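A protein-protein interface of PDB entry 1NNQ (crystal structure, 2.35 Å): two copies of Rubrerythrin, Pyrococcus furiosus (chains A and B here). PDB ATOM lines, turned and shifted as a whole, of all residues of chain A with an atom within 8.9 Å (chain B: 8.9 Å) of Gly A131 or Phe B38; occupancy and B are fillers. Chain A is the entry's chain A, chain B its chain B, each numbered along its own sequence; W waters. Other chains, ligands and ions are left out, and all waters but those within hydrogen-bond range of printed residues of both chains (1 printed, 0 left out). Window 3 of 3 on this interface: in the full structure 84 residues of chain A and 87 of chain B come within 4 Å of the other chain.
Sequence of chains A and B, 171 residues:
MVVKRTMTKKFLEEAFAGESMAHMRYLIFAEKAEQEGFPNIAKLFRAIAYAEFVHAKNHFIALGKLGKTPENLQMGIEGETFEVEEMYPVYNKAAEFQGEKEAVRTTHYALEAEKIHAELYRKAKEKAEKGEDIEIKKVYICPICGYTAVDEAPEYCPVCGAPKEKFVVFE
No position is printed for both chains.
The backbone carbonyl oxygen (O) of Lys A68 sits close to the side-chain amide nitrogen (ND2) of Asn A72, 3.4 Å away. The backbone carbonyl oxygen of Lys A127 lies within hydrogen-bond range of the backbone NH of Glu A132 (3.0 Å). The backbone NH (N) of Phe B38 lies within hydrogen-bond range of the backbone carbonyl oxygen (O) of Ala B33, 2.8 Å away.
Water W1 lies within hydrogen-bond range of the side-chain amide nitrogen of Asn A72 (2.7 Å), the backbone carbonyl oxygen of Phe B29 (2.8 Å) and the side-chain hydroxyl of Thr A69 (2.8 Å).
Of the 17 printed residues of chain B, 10 touch a printed residue of chain A. Printed residues of chain B that touch a printed residue of chain A: Phe B29, Lys B32, Ala B33, Glu B36, Phe B38, Pro B39, Asn B40, Ile B41, Leu B44 and Phe B45. Hydrophobic or aromatic side chains of chain B within 4 Å of the printed part of chain A: Phe B29, Ala B33, Phe B38, Pro B39, Ile B41, Leu B44 and Phe B45. Along chain B the printed residues that touch a printed residue of chain A span positions 29 to 45. Of the 18 printed residues of chain A, 10 touch a printed residue of chain B. Hydrophobic or aromatic side chains of chain A within 4 Å of the printed part of chain B: Leu A73, Ala A128, Ile A134 and Ile A136. Among the printed residues, 19 pairs touch across the chains. Among the printed residues, no Asp or Glu carboxylate lies within 4 Å of a Lys or Arg side-chain nitrogen of the other chain.
The backbone NH of Thr A69 is in hydrogen-bond range of the side-chain carboxylate of Glu B36 (2.8 Å). The side-chain carboxylate (OD1) of Asp A133 sits at hydrogen-bond distance from the backbone NH (N) of Asn B40 (2.9 Å). The side-chain carboxylate (OD2) of Asp A133 is in hydrogen-bond range of the backbone NH (N) of Ile B41 (3.0 Å). O of Ile A134 is in hydrogen-bond range of ND2 of Asn B40, at 2.7 Å. N of Pro B39 sits close to OD1 of Asp A133.
Of chain B, only Phe B38 comes within 4 Å of Gly A131. Printed residues of chain A within 4 Å of Phe B38: Thr A69 (3.7 Å), Gly A131 (3.8 Å), Glu A132 (3.9 Å) and Asp A133 (3.5 Å). No residue of chain A comes within 4 Å of Gly B37. Printed residues of chain B within 4 Å of Thr A69: Ala B33, Glu B36, Phe B38 and Ile B41. Printed residues of chain A within 4 Å of Phe B45: Leu A73 (3.5 Å). Of the printed residues of chain B, Leu A73 touches Phe B45. Of the printed residues of chain B, Glu A132 touches Phe B38 (3.9 Å). Of the printed residues of chain A, Ile B41 touches Thr A69, Ala A128, Asp A133 and Ile A134. The nearest residue of chain B that does not touch Gly A131 is Gly B37 (6.0 Å). The nearest residue of chain A that does not touch Phe B38 is Ala A128 (4.03 Å). The nearest printed residue of chain B that does not touch Leu A73 is Ile B41 (4.3 Å).
Glu B36 touches Lys A68 (OE2 to CG, 3.4 Å). Ala B33 touches Thr A69. O of Asn A72 touches CE1 of Phe B29 (3.4 Å). Lys B32 touches Asn A72 (CG to ND2, 3.9 Å). Leu A73 touches Phe B45. O of Gly A131 touches CE2 of Phe B38, 3.8 Å away. C of Phe B38 touches OD1 of Asp A133 (3.5 Å). Ile A134 touches Ile B41 (CG1 to CG1, 3.8 Å). Leu B44 touches Ile A134 (CD2 to CD1, 3.9 Å). ND2 of Asn B40 touches N of Ile A136, at 3.8 Å.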
ATOM      1  N   LYS A  68     -10.630  -3.885 -17.096  1.00  0.00           N
ATOM      2  CA  LYS A  68      -9.936  -3.482 -15.886  1.00  0.00           C
ATOM      3  C   LYS A  68      -8.522  -3.013 -16.208  1.00  0.00           C
ATOM      4  O   LYS A  68      -7.927  -3.407 -17.232  1.00  0.00           O
ATOM      5  CB  LYS A  68      -9.852  -4.647 -14.897  1.00  0.00           C
ATOM      6  CG  LYS A  68     -11.171  -5.044 -14.226  1.00  0.00           C
ATOM      7  CD  LYS A  68     -11.006  -6.428 -13.599  1.00  0.00           C
ATOM      8  CE  LYS A  68     -12.291  -6.918 -12.939  1.00  0.00           C
ATOM      9  NZ  LYS A  68     -12.232  -8.404 -12.694  1.00  0.00           N
ATOM     10  N   THR A  69      -7.967  -2.210 -15.305  1.00  0.00           N
ATOM     11  CA  THR A  69      -6.635  -1.664 -15.491  1.00  0.00           C
ATOM     12  C   THR A  69      -5.562  -2.655 -15.979  1.00  0.00           C
ATOM     13  O   THR A  69      -4.827  -2.307 -16.895  1.00  0.00           O
ATOM     14  CB  THR A  69      -6.211  -0.839 -14.251  1.00  0.00           C
ATOM     15  OG1 THR A  69      -6.994   0.366 -14.221  1.00  0.00           O
ATOM     16  CG2 THR A  69      -4.778  -0.324 -14.370  1.00  0.00           C
ATOM     17  N   PRO A  70      -5.460  -3.870 -15.429  1.00  0.00           N
ATOM     18  CA  PRO A  70      -4.444  -4.808 -15.934  1.00  0.00           C
ATOM     19  C   PRO A  70      -4.668  -5.209 -17.398  1.00  0.00           C
ATOM     20  O   PRO A  70      -3.702  -5.339 -18.152  1.00  0.00           O
ATOM     21  CB  PRO A  70      -4.582  -6.027 -14.993  1.00  0.00           C
ATOM     22  CG  PRO A  70      -5.322  -5.493 -13.778  1.00  0.00           C
ATOM     23  CD  PRO A  70      -6.230  -4.458 -14.305  1.00  0.00           C
ATOM     24  N   GLU A  71      -5.915  -5.399 -17.802  1.00  0.00           N
ATOM     25  CA  GLU A  71      -6.183  -5.739 -19.199  1.00  0.00           C
ATOM     26  C   GLU A  71      -5.927  -4.528 -20.124  1.00  0.00           C
ATOM     27  O   GLU A  71      -5.401  -4.674 -21.234  1.00  0.00           O
ATOM     28  CB  GLU A  71      -7.608  -6.268 -19.383  1.00  0.00           C
ATOM     29  N   ASN A  72      -6.318  -3.347 -19.662  1.00  0.00           N
ATOM     30  CA  ASN A  72      -6.099  -2.118 -20.406  1.00  0.00           C
ATOM     31  C   ASN A  72      -4.601  -1.971 -20.636  1.00  0.00           C
ATOM     32  O   ASN A  72      -4.162  -1.683 -21.743  1.00  0.00           O
ATOM     33  CB  ASN A  72      -6.658  -0.924 -19.643  1.00  0.00           C
ATOM     34  CG  ASN A  72      -8.164  -1.019 -19.412  1.00  0.00           C
ATOM     35  OD1 ASN A  72      -8.891  -1.693 -20.153  1.00  0.00           O
ATOM     36  ND2 ASN A  72      -8.646  -0.317 -18.398  1.00  0.00           N
ATOM     37  N   LEU A  73      -3.820  -2.235 -19.590  1.00  0.00           N
ATOM     38  CA  LEU A  73      -2.370  -2.159 -19.680  1.00  0.00           C
ATOM     39  C   LEU A  73      -1.822  -3.161 -20.691  1.00  0.00           C
ATOM     40  O   LEU A  73      -0.914  -2.827 -21.452  1.00  0.00           O
ATOM     41  CB  LEU A  73      -1.731  -2.357 -18.302  1.00  0.00           C
ATOM     42  CG  LEU A  73      -1.784  -1.157 -17.341  1.00  0.00           C
ATOM     43  CD1 LEU A  73      -1.539  -1.630 -15.910  1.00  0.00           C
ATOM     44  CD2 LEU A  73      -0.770  -0.055 -17.731  1.00  0.00           C
ATOM     45  N   ALA A 124       4.129  -1.548 -15.034  1.00  0.00           N
ATOM     46  CA  ALA A 124       2.924  -1.164 -14.280  1.00  0.00           C
ATOM     47  C   ALA A 124       1.941  -2.308 -14.137  1.00  0.00           C
ATOM     48  O   ALA A 124       1.205  -2.356 -13.151  1.00  0.00           O
ATOM     49  CB  ALA A 124       2.214   0.054 -14.896  1.00  0.00           C
ATOM     50  N   LYS A 125       1.922  -3.207 -15.126  1.00  0.00           N
ATOM     51  CA  LYS A 125       0.975  -4.328 -15.135  1.00  0.00           C
ATOM     52  C   LYS A 125       1.257  -5.355 -14.025  1.00  0.00           C
ATOM     53  O   LYS A 125       0.327  -5.838 -13.389  1.00  0.00           O
ATOM     54  CB  LYS A 125       0.870  -5.007 -16.519  1.00  0.00           C
ATOM     55  CG  LYS A 125      -0.416  -5.783 -16.705  1.00  0.00           C
ATOM     56  CD  LYS A 125      -0.256  -6.894 -17.751  1.00  0.00           C
ATOM     57  CE  LYS A 125      -1.361  -7.941 -17.646  1.00  0.00           C
ATOM     58  NZ  LYS A 125      -1.130  -9.120 -18.579  1.00  0.00           N
ATOM     59  N   GLU A 126       2.533  -5.674 -13.811  1.00  0.00           N
ATOM     60  CA  GLU A 126       2.967  -6.466 -12.660  1.00  0.00           C
ATOM     61  C   GLU A 126       2.318  -5.930 -11.380  1.00  0.00           C
ATOM     62  O   GLU A 126       1.715  -6.684 -10.595  1.00  0.00           O
ATOM     63  CB  GLU A 126       4.489  -6.411 -12.530  1.00  0.00           C
ATOM     64  CG  GLU A 126       5.234  -7.651 -13.007  1.00  0.00           C
ATOM     65  CD  GLU A 126       6.717  -7.612 -12.652  1.00  0.00           C
ATOM     66  OE1 GLU A 126       7.136  -8.377 -11.745  1.00  0.00           O
ATOM     67  OE2 GLU A 126       7.463  -6.816 -13.277  1.00  0.00           O
ATOM     68  N   LYS A 127       2.427  -4.616 -11.197  1.00  0.00           N
ATOM     69  CA  LYS A 127       1.864  -3.947 -10.035  1.00  0.00           C
ATOM     70  C   LYS A 127       0.332  -4.060 -10.000  1.00  0.00           C
ATOM     71  O   LYS A 127      -0.212  -4.590  -9.034  1.00  0.00           O
ATOM     72  CB  LYS A 127       2.338  -2.491  -9.967  1.00  0.00           C
ATOM     73  CG  LYS A 127       3.854  -2.340  -9.895  1.00  0.00           C
ATOM     74  N   ALA A 128      -0.349  -3.603 -11.052  1.00  0.00           N
ATOM     75  CA  ALA A 128      -1.816  -3.583 -11.081  1.00  0.00           C
ATOM     76  C   ALA A 128      -2.449  -4.956 -10.856  1.00  0.00           C
ATOM     77  O   ALA A 128      -3.471  -5.069 -10.170  1.00  0.00           O
ATOM     78  CB  ALA A 128      -2.331  -2.982 -12.396  1.00  0.00           C
ATOM     79  N   GLU A 129      -1.845  -5.979 -11.459  1.00  0.00           N
ATOM     80  CA  GLU A 129      -2.309  -7.355 -11.331  1.00  0.00           C
ATOM     81  C   GLU A 129      -2.279  -7.859  -9.869  1.00  0.00           C
ATOM     82  O   GLU A 129      -3.111  -8.680  -9.483  1.00  0.00           O
ATOM     83  CB  GLU A 129      -1.489  -8.271 -12.240  1.00  0.00           C
ATOM     84  N   LYS A 130      -1.322  -7.355  -9.079  1.00  0.00           N
ATOM     85  CA  LYS A 130      -1.193  -7.662  -7.647  1.00  0.00           C
ATOM     86  C   LYS A 130      -1.997  -6.686  -6.789  1.00  0.00           C
ATOM     87  O   LYS A 130      -1.811  -6.622  -5.574  1.00  0.00           O
ATOM     88  CB  LYS A 130       0.271  -7.590  -7.210  1.00  0.00           C
ATOM     89  CG  LYS A 130       1.113  -8.816  -7.523  1.00  0.00           C
ATOM     90  CD  LYS A 130       2.530  -8.684  -6.928  1.00  0.00           C
ATOM     91  CE  LYS A 130       3.113  -7.274  -7.093  1.00  0.00           C
ATOM     92  NZ  LYS A 130       4.607  -7.247  -7.073  1.00  0.00           N
ATOM     93  N   GLY A 131      -2.867  -5.910  -7.432  1.00  0.00           N
ATOM     94  CA  GLY A 131      -3.699  -4.921  -6.758  1.00  0.00           C
ATOM     95  C   GLY A 131      -2.934  -3.715  -6.220  1.00  0.00           C
ATOM     96  O   GLY A 131      -3.517  -2.893  -5.503  1.00  0.00           O
ATOM     97  N   GLU A 132      -1.641  -3.620  -6.542  1.00  0.00           N
ATOM     98  CA  GLU A 132      -0.799  -2.487  -6.154  1.00  0.00           C
ATOM     99  C   GLU A 132      -0.764  -1.400  -7.253  1.00  0.00           C
ATOM    100  O   GLU A 132      -0.520  -1.699  -8.419  1.00  0.00           O
ATOM    101  CB  GLU A 132       0.643  -2.961  -5.865  1.00  0.00           C
ATOM    102  CG  GLU A 132       0.850  -3.842  -4.622  1.00  0.00           C
ATOM    103  CD  GLU A 132       2.305  -4.307  -4.430  1.00  0.00           C
ATOM    104  OE1 GLU A 132       2.538  -5.294  -3.684  1.00  0.00           O
ATOM    105  OE2 GLU A 132       3.236  -3.693  -5.012  1.00  0.00           O
ATOM    106  N   ASP A 133      -1.014  -0.144  -6.879  1.00  0.00           N
ATOM    107  CA  ASP A 133      -0.664   0.996  -7.732  1.00  0.00           C
ATOM    108  C   ASP A 133       0.856   1.060  -7.906  1.00  0.00           C
ATOM    109  O   ASP A 133       1.587   0.497  -7.098  1.00  0.00           O
ATOM    110  CB  ASP A 133      -1.166   2.314  -7.134  1.00  0.00           C
ATOM    111  CG  ASP A 133      -1.216   3.444  -8.163  1.00  0.00           C
ATOM    112  OD1 ASP A 133      -1.474   4.598  -7.783  1.00  0.00           O
ATOM    113  OD2 ASP A 133      -1.008   3.279  -9.381  1.00  0.00           O
ATOM    114  N   ILE A 134       1.336   1.719  -8.960  1.00  0.00           N
ATOM    115  CA  ILE A 134       2.783   1.921  -9.111  1.00  0.00           C
ATOM    116  C   ILE A 134       3.223   3.069  -8.208  1.00  0.00           C
ATOM    117  O   ILE A 134       2.402   3.885  -7.787  1.00  0.00           O
ATOM    118  CB  ILE A 134       3.206   2.205 -10.588  1.00  0.00           C
ATOM    119  CG1 ILE A 134       2.520   3.472 -11.126  1.00  0.00           C
ATOM    120  CG2 ILE A 134       2.945   1.001 -11.440  1.00  0.00           C
ATOM    121  CD1 ILE A 134       2.970   3.874 -12.520  1.00  0.00           C
ATOM    122  N   ILE A 136       5.362   6.252  -8.261  1.00  0.00           N
ATOM    123  CA  ILE A 136       6.076   7.247  -9.063  1.00  0.00           C
ATOM    124  C   ILE A 136       5.770   8.672  -8.600  1.00  0.00           C
ATOM    125  O   ILE A 136       4.644   8.981  -8.202  1.00  0.00           O
ATOM    126  CB  ILE A 136       5.819   7.076 -10.607  1.00  0.00           C
ATOM    127  CG1 ILE A 136       4.369   7.410 -10.986  1.00  0.00           C
ATOM    128  CG2 ILE A 136       6.211   5.677 -11.086  1.00  0.00           C
ATOM    129  CD1 ILE A 136       4.123   7.463 -12.497  1.00  0.00           C
ATOM    130  N   PHE B  29      -8.362   4.935 -20.560  1.00  0.00           N
ATOM    131  CA  PHE B  29      -7.790   4.037 -19.574  1.00  0.00           C
ATOM    132  C   PHE B  29      -7.432   4.797 -18.307  1.00  0.00           C
ATOM    133  O   PHE B  29      -7.469   4.214 -17.232  1.00  0.00           O
ATOM    134  CB  PHE B  29      -6.544   3.333 -20.110  1.00  0.00           C
ATOM    135  CG  PHE B  29      -6.817   2.321 -21.196  1.00  0.00           C
ATOM    136  CD1 PHE B  29      -5.776   1.885 -22.016  1.00  0.00           C
ATOM    137  CD2 PHE B  29      -8.089   1.811 -21.409  1.00  0.00           C
ATOM    138  CE1 PHE B  29      -5.991   0.947 -23.007  1.00  0.00           C
ATOM    139  CE2 PHE B  29      -8.311   0.864 -22.407  1.00  0.00           C
ATOM    140  CZ  PHE B  29      -7.260   0.430 -23.201  1.00  0.00           C
ATOM    141  N   ALA B  30      -7.067   6.078 -18.441  1.00  0.00           N
ATOM    142  CA  ALA B  30      -6.645   6.911 -17.314  1.00  0.00           C
ATOM    143  C   ALA B  30      -7.786   7.056 -16.337  1.00  0.00           C
ATOM    144  O   ALA B  30      -7.628   6.828 -15.127  1.00  0.00           O
ATOM    145  CB  ALA B  30      -6.235   8.291 -17.792  1.00  0.00           C
ATOM    146  N   GLU B  31      -8.928   7.451 -16.901  1.00  0.00           N
ATOM    147  CA  GLU B  31     -10.158   7.682 -16.180  1.00  0.00           C
ATOM    148  C   GLU B  31     -10.576   6.383 -15.465  1.00  0.00           C
ATOM    149  O   GLU B  31     -10.978   6.415 -14.311  1.00  0.00           O
ATOM    150  CB  GLU B  31     -11.211   8.181 -17.181  1.00  0.00           C
ATOM    151  CG  GLU B  31     -12.402   8.928 -16.608  1.00  0.00           C
ATOM    152  CD  GLU B  31     -13.509   9.183 -17.641  1.00  0.00           C
ATOM    153  OE1 GLU B  31     -14.262  10.170 -17.483  1.00  0.00           O
ATOM    154  OE2 GLU B  31     -13.643   8.397 -18.610  1.00  0.00           O
ATOM    155  N   LYS B  32     -10.435   5.243 -16.133  1.00  0.00           N
ATOM    156  CA  LYS B  32     -10.745   3.954 -15.523  1.00  0.00           C
ATOM    157  C   LYS B  32      -9.767   3.569 -14.406  1.00  0.00           C
ATOM    158  O   LYS B  32     -10.157   2.949 -13.412  1.00  0.00           O
ATOM    159  CB  LYS B  32     -10.826   2.844 -16.579  1.00  0.00           C
ATOM    160  CG  LYS B  32     -11.209   1.460 -16.023  1.00  0.00           C
ATOM    161  CD  LYS B  32     -12.604   1.462 -15.394  1.00  0.00           C
ATOM    162  CE  LYS B  32     -13.441   0.297 -15.905  1.00  0.00           C
ATOM    163  NZ  LYS B  32     -14.281  -0.315 -14.828  1.00  0.00           N
ATOM    164  N   ALA B  33      -8.499   3.922 -14.576  1.00  0.00           N
ATOM    165  CA  ALA B  33      -7.491   3.574 -13.590  1.00  0.00           C
ATOM    166  C   ALA B  33      -7.751   4.339 -12.289  1.00  0.00           C
ATOM    167  O   ALA B  33      -7.625   3.765 -11.207  1.00  0.00           O
ATOM    168  CB  ALA B  33      -6.100   3.825 -14.116  1.00  0.00           C
ATOM    169  N   GLU B  34      -8.164   5.607 -12.400  1.00  0.00           N
ATOM    170  CA  GLU B  34      -8.478   6.420 -11.226  1.00  0.00           C
ATOM    171  C   GLU B  34      -9.679   5.844 -10.462  1.00  0.00           C
ATOM    172  O   GLU B  34      -9.595   5.632  -9.248  1.00  0.00           O
ATOM    173  CB  GLU B  34      -8.714   7.883 -11.612  1.00  0.00           C
ATOM    174  N   GLN B  35     -10.771   5.562 -11.186  1.00  0.00           N
ATOM    175  CA  GLN B  35     -11.964   4.912 -10.628  1.00  0.00           C
ATOM    176  C   GLN B  35     -11.633   3.606  -9.878  1.00  0.00           C
ATOM    177  O   GLN B  35     -12.256   3.303  -8.864  1.00  0.00           O
ATOM    178  CB  GLN B  35     -13.040   4.667 -11.716  1.00  0.00           C
ATOM    179  CG  GLN B  35     -13.685   5.964 -12.285  1.00  0.00           C
ATOM    180  CD  GLN B  35     -14.422   5.791 -13.639  1.00  0.00           C
ATOM    181  OE1 GLN B  35     -14.442   4.701 -14.225  1.00  0.00           O
ATOM    182  NE2 GLN B  35     -15.032   6.878 -14.123  1.00  0.00           N
ATOM    183  N   GLU B  36     -10.642   2.856 -10.365  1.00  0.00           N
ATOM    184  CA  GLU B  36     -10.237   1.592  -9.734  1.00  0.00           C
ATOM    185  C   GLU B  36      -9.224   1.759  -8.580  1.00  0.00           C
ATOM    186  O   GLU B  36      -8.784   0.771  -7.988  1.00  0.00           O
ATOM    187  CB  GLU B  36      -9.702   0.603 -10.782  1.00  0.00           C
ATOM    188  CG  GLU B  36     -10.772  -0.171 -11.545  1.00  0.00           C
ATOM    189  CD  GLU B  36     -10.181  -1.220 -12.487  1.00  0.00           C
ATOM    190  OE1 GLU B  36      -9.567  -0.851 -13.502  1.00  0.00           O
ATOM    191  OE2 GLU B  36     -10.310  -2.426 -12.226  1.00  0.00           O
ATOM    192  N   GLY B  37      -8.873   3.006  -8.253  1.00  0.00           N
ATOM    193  CA  GLY B  37      -7.905   3.290  -7.197  1.00  0.00           C
ATOM    194  C   GLY B  37      -6.446   3.073  -7.597  1.00  0.00           C
ATOM    195  O   GLY B  37      -5.641   2.566  -6.801  1.00  0.00           O
ATOM    196  N   PHE B  38      -6.096   3.472  -8.826  1.00  0.00           N
ATOM    197  CA  PHE B  38      -4.704   3.468  -9.281  1.00  0.00           C
ATOM    198  C   PHE B  38      -4.315   4.855  -9.802  1.00  0.00           C
ATOM    199  O   PHE B  38      -4.056   4.997 -11.003  1.00  0.00           O
ATOM    200  CB  PHE B  38      -4.493   2.448 -10.401  1.00  0.00           C
ATOM    201  CG  PHE B  38      -4.820   1.032 -10.029  1.00  0.00           C
ATOM    202  CD1 PHE B  38      -5.834   0.355 -10.680  1.00  0.00           C
ATOM    203  CD2 PHE B  38      -4.077   0.358  -9.064  1.00  0.00           C
ATOM    204  CE1 PHE B  38      -6.126  -0.964 -10.358  1.00  0.00           C
ATOM    205  CE2 PHE B  38      -4.366  -0.963  -8.721  1.00  0.00           C
ATOM    206  CZ  PHE B  38      -5.397  -1.624  -9.366  1.00  0.00           C
ATOM    207  N   PRO B  39      -4.242   5.870  -8.932  1.00  0.00           N
ATOM    208  CA  PRO B  39      -4.002   7.251  -9.395  1.00  0.00           C
ATOM    209  C   PRO B  39      -2.660   7.441 -10.109  1.00  0.00           C
ATOM    210  O   PRO B  39      -2.572   8.234 -11.043  1.00  0.00           O
ATOM    211  CB  PRO B  39      -4.062   8.094  -8.108  1.00  0.00           C
ATOM    212  CG  PRO B  39      -3.773   7.115  -6.979  1.00  0.00           C
ATOM    213  CD  PRO B  39      -4.343   5.788  -7.458  1.00  0.00           C
ATOM    214  N   ASN B  40      -1.634   6.724  -9.678  1.00  0.00           N
ATOM    215  CA  ASN B  40      -0.338   6.793 -10.336  1.00  0.00           C
ATOM    216  C   ASN B  40      -0.329   6.152 -11.728  1.00  0.00           C
ATOM    217  O   ASN B  40       0.278   6.679 -12.645  1.00  0.00           O
ATOM    218  CB  ASN B  40       0.760   6.196  -9.447  1.00  0.00           C
ATOM    219  CG  ASN B  40       1.059   7.056  -8.224  1.00  0.00           C
ATOM    220  OD1 ASN B  40       0.716   8.245  -8.179  1.00  0.00           O
ATOM    221  ND2 ASN B  40       1.711   6.458  -7.223  1.00  0.00           N
ATOM    222  N   ILE B  41      -0.991   5.014 -11.889  1.00  0.00           N
ATOM    223  CA  ILE B  41      -1.143   4.428 -13.213  1.00  0.00           C
ATOM    224  C   ILE B  41      -1.943   5.359 -14.130  1.00  0.00           C
ATOM    225  O   ILE B  41      -1.599   5.504 -15.317  1.00  0.00           O
ATOM    226  CB  ILE B  41      -1.783   3.022 -13.127  1.00  0.00           C
ATOM    227  CG1 ILE B  41      -0.810   2.062 -12.429  1.00  0.00           C
ATOM    228  CG2 ILE B  41      -2.148   2.498 -14.522  1.00  0.00           C
ATOM    229  CD1 ILE B  41      -1.338   0.657 -12.250  1.00  0.00           C
ATOM    230  N   ALA B  42      -3.002   5.970 -13.583  1.00  0.00           N
ATOM    231  CA  ALA B  42      -3.740   7.022 -14.282  1.00  0.00           C
ATOM    232  C   ALA B  42      -2.793   8.156 -14.756  1.00  0.00           C
ATOM    233  O   ALA B  42      -2.832   8.551 -15.927  1.00  0.00           O
ATOM    234  CB  ALA B  42      -4.857   7.575 -13.402  1.00  0.00           C
ATOM    235  N   LYS B  43      -1.937   8.648 -13.851  1.00  0.00           N
ATOM    236  CA  LYS B  43      -0.926   9.653 -14.181  1.00  0.00           C
ATOM    237  C   LYS B  43      -0.019   9.195 -15.332  1.00  0.00           C
ATOM    238  O   LYS B  43       0.299   9.990 -16.237  1.00  0.00           O
ATOM    239  CB  LYS B  43      -0.092  10.012 -12.948  1.00  0.00           C
ATOM    240  CG  LYS B  43       0.847  11.216 -13.146  1.00  0.00           C
ATOM    241  N   LEU B  44       0.367   7.917 -15.314  1.00  0.00           N
ATOM    242  CA  LEU B  44       1.220   7.351 -16.353  1.00  0.00           C
ATOM    243  C   LEU B  44       0.500   7.268 -17.692  1.00  0.00           C
ATOM    244  O   LEU B  44       1.081   7.560 -18.726  1.00  0.00           O
ATOM    245  CB  LEU B  44       1.735   5.966 -15.940  1.00  0.00           C
ATOM    246  CG  LEU B  44       2.675   5.224 -16.907  1.00  0.00           C
ATOM    247  CD1 LEU B  44       4.008   5.958 -17.045  1.00  0.00           C
ATOM    248  CD2 LEU B  44       2.915   3.789 -16.436  1.00  0.00           C
ATOM    249  N   PHE B  45      -0.766   6.865 -17.665  1.00  0.00           N
ATOM    250  CA  PHE B  45      -1.615   6.889 -18.857  1.00  0.00           C
ATOM    251  C   PHE B  45      -1.711   8.281 -19.475  1.00  0.00           C
ATOM    252  O   PHE B  45      -1.557   8.411 -20.703  1.00  0.00           O
ATOM    253  CB  PHE B  45      -3.033   6.360 -18.558  1.00  0.00           C
ATOM    254  CG  PHE B  45      -3.153   4.862 -18.636  1.00  0.00           C
ATOM    255  CD1 PHE B  45      -2.696   4.161 -19.764  1.00  0.00           C
ATOM    256  CD2 PHE B  45      -3.726   4.140 -17.583  1.00  0.00           C
ATOM    257  CE1 PHE B  45      -2.809   2.769 -19.845  1.00  0.00           C
ATOM    258  CE2 PHE B  45      -3.846   2.746 -17.654  1.00  0.00           C
ATOM    259  CZ  PHE B  45      -3.378   2.057 -18.785  1.00  0.00           C
HETATM  260  O   HOH W   1      -7.306   1.457 -16.828  1.00  0.00           O
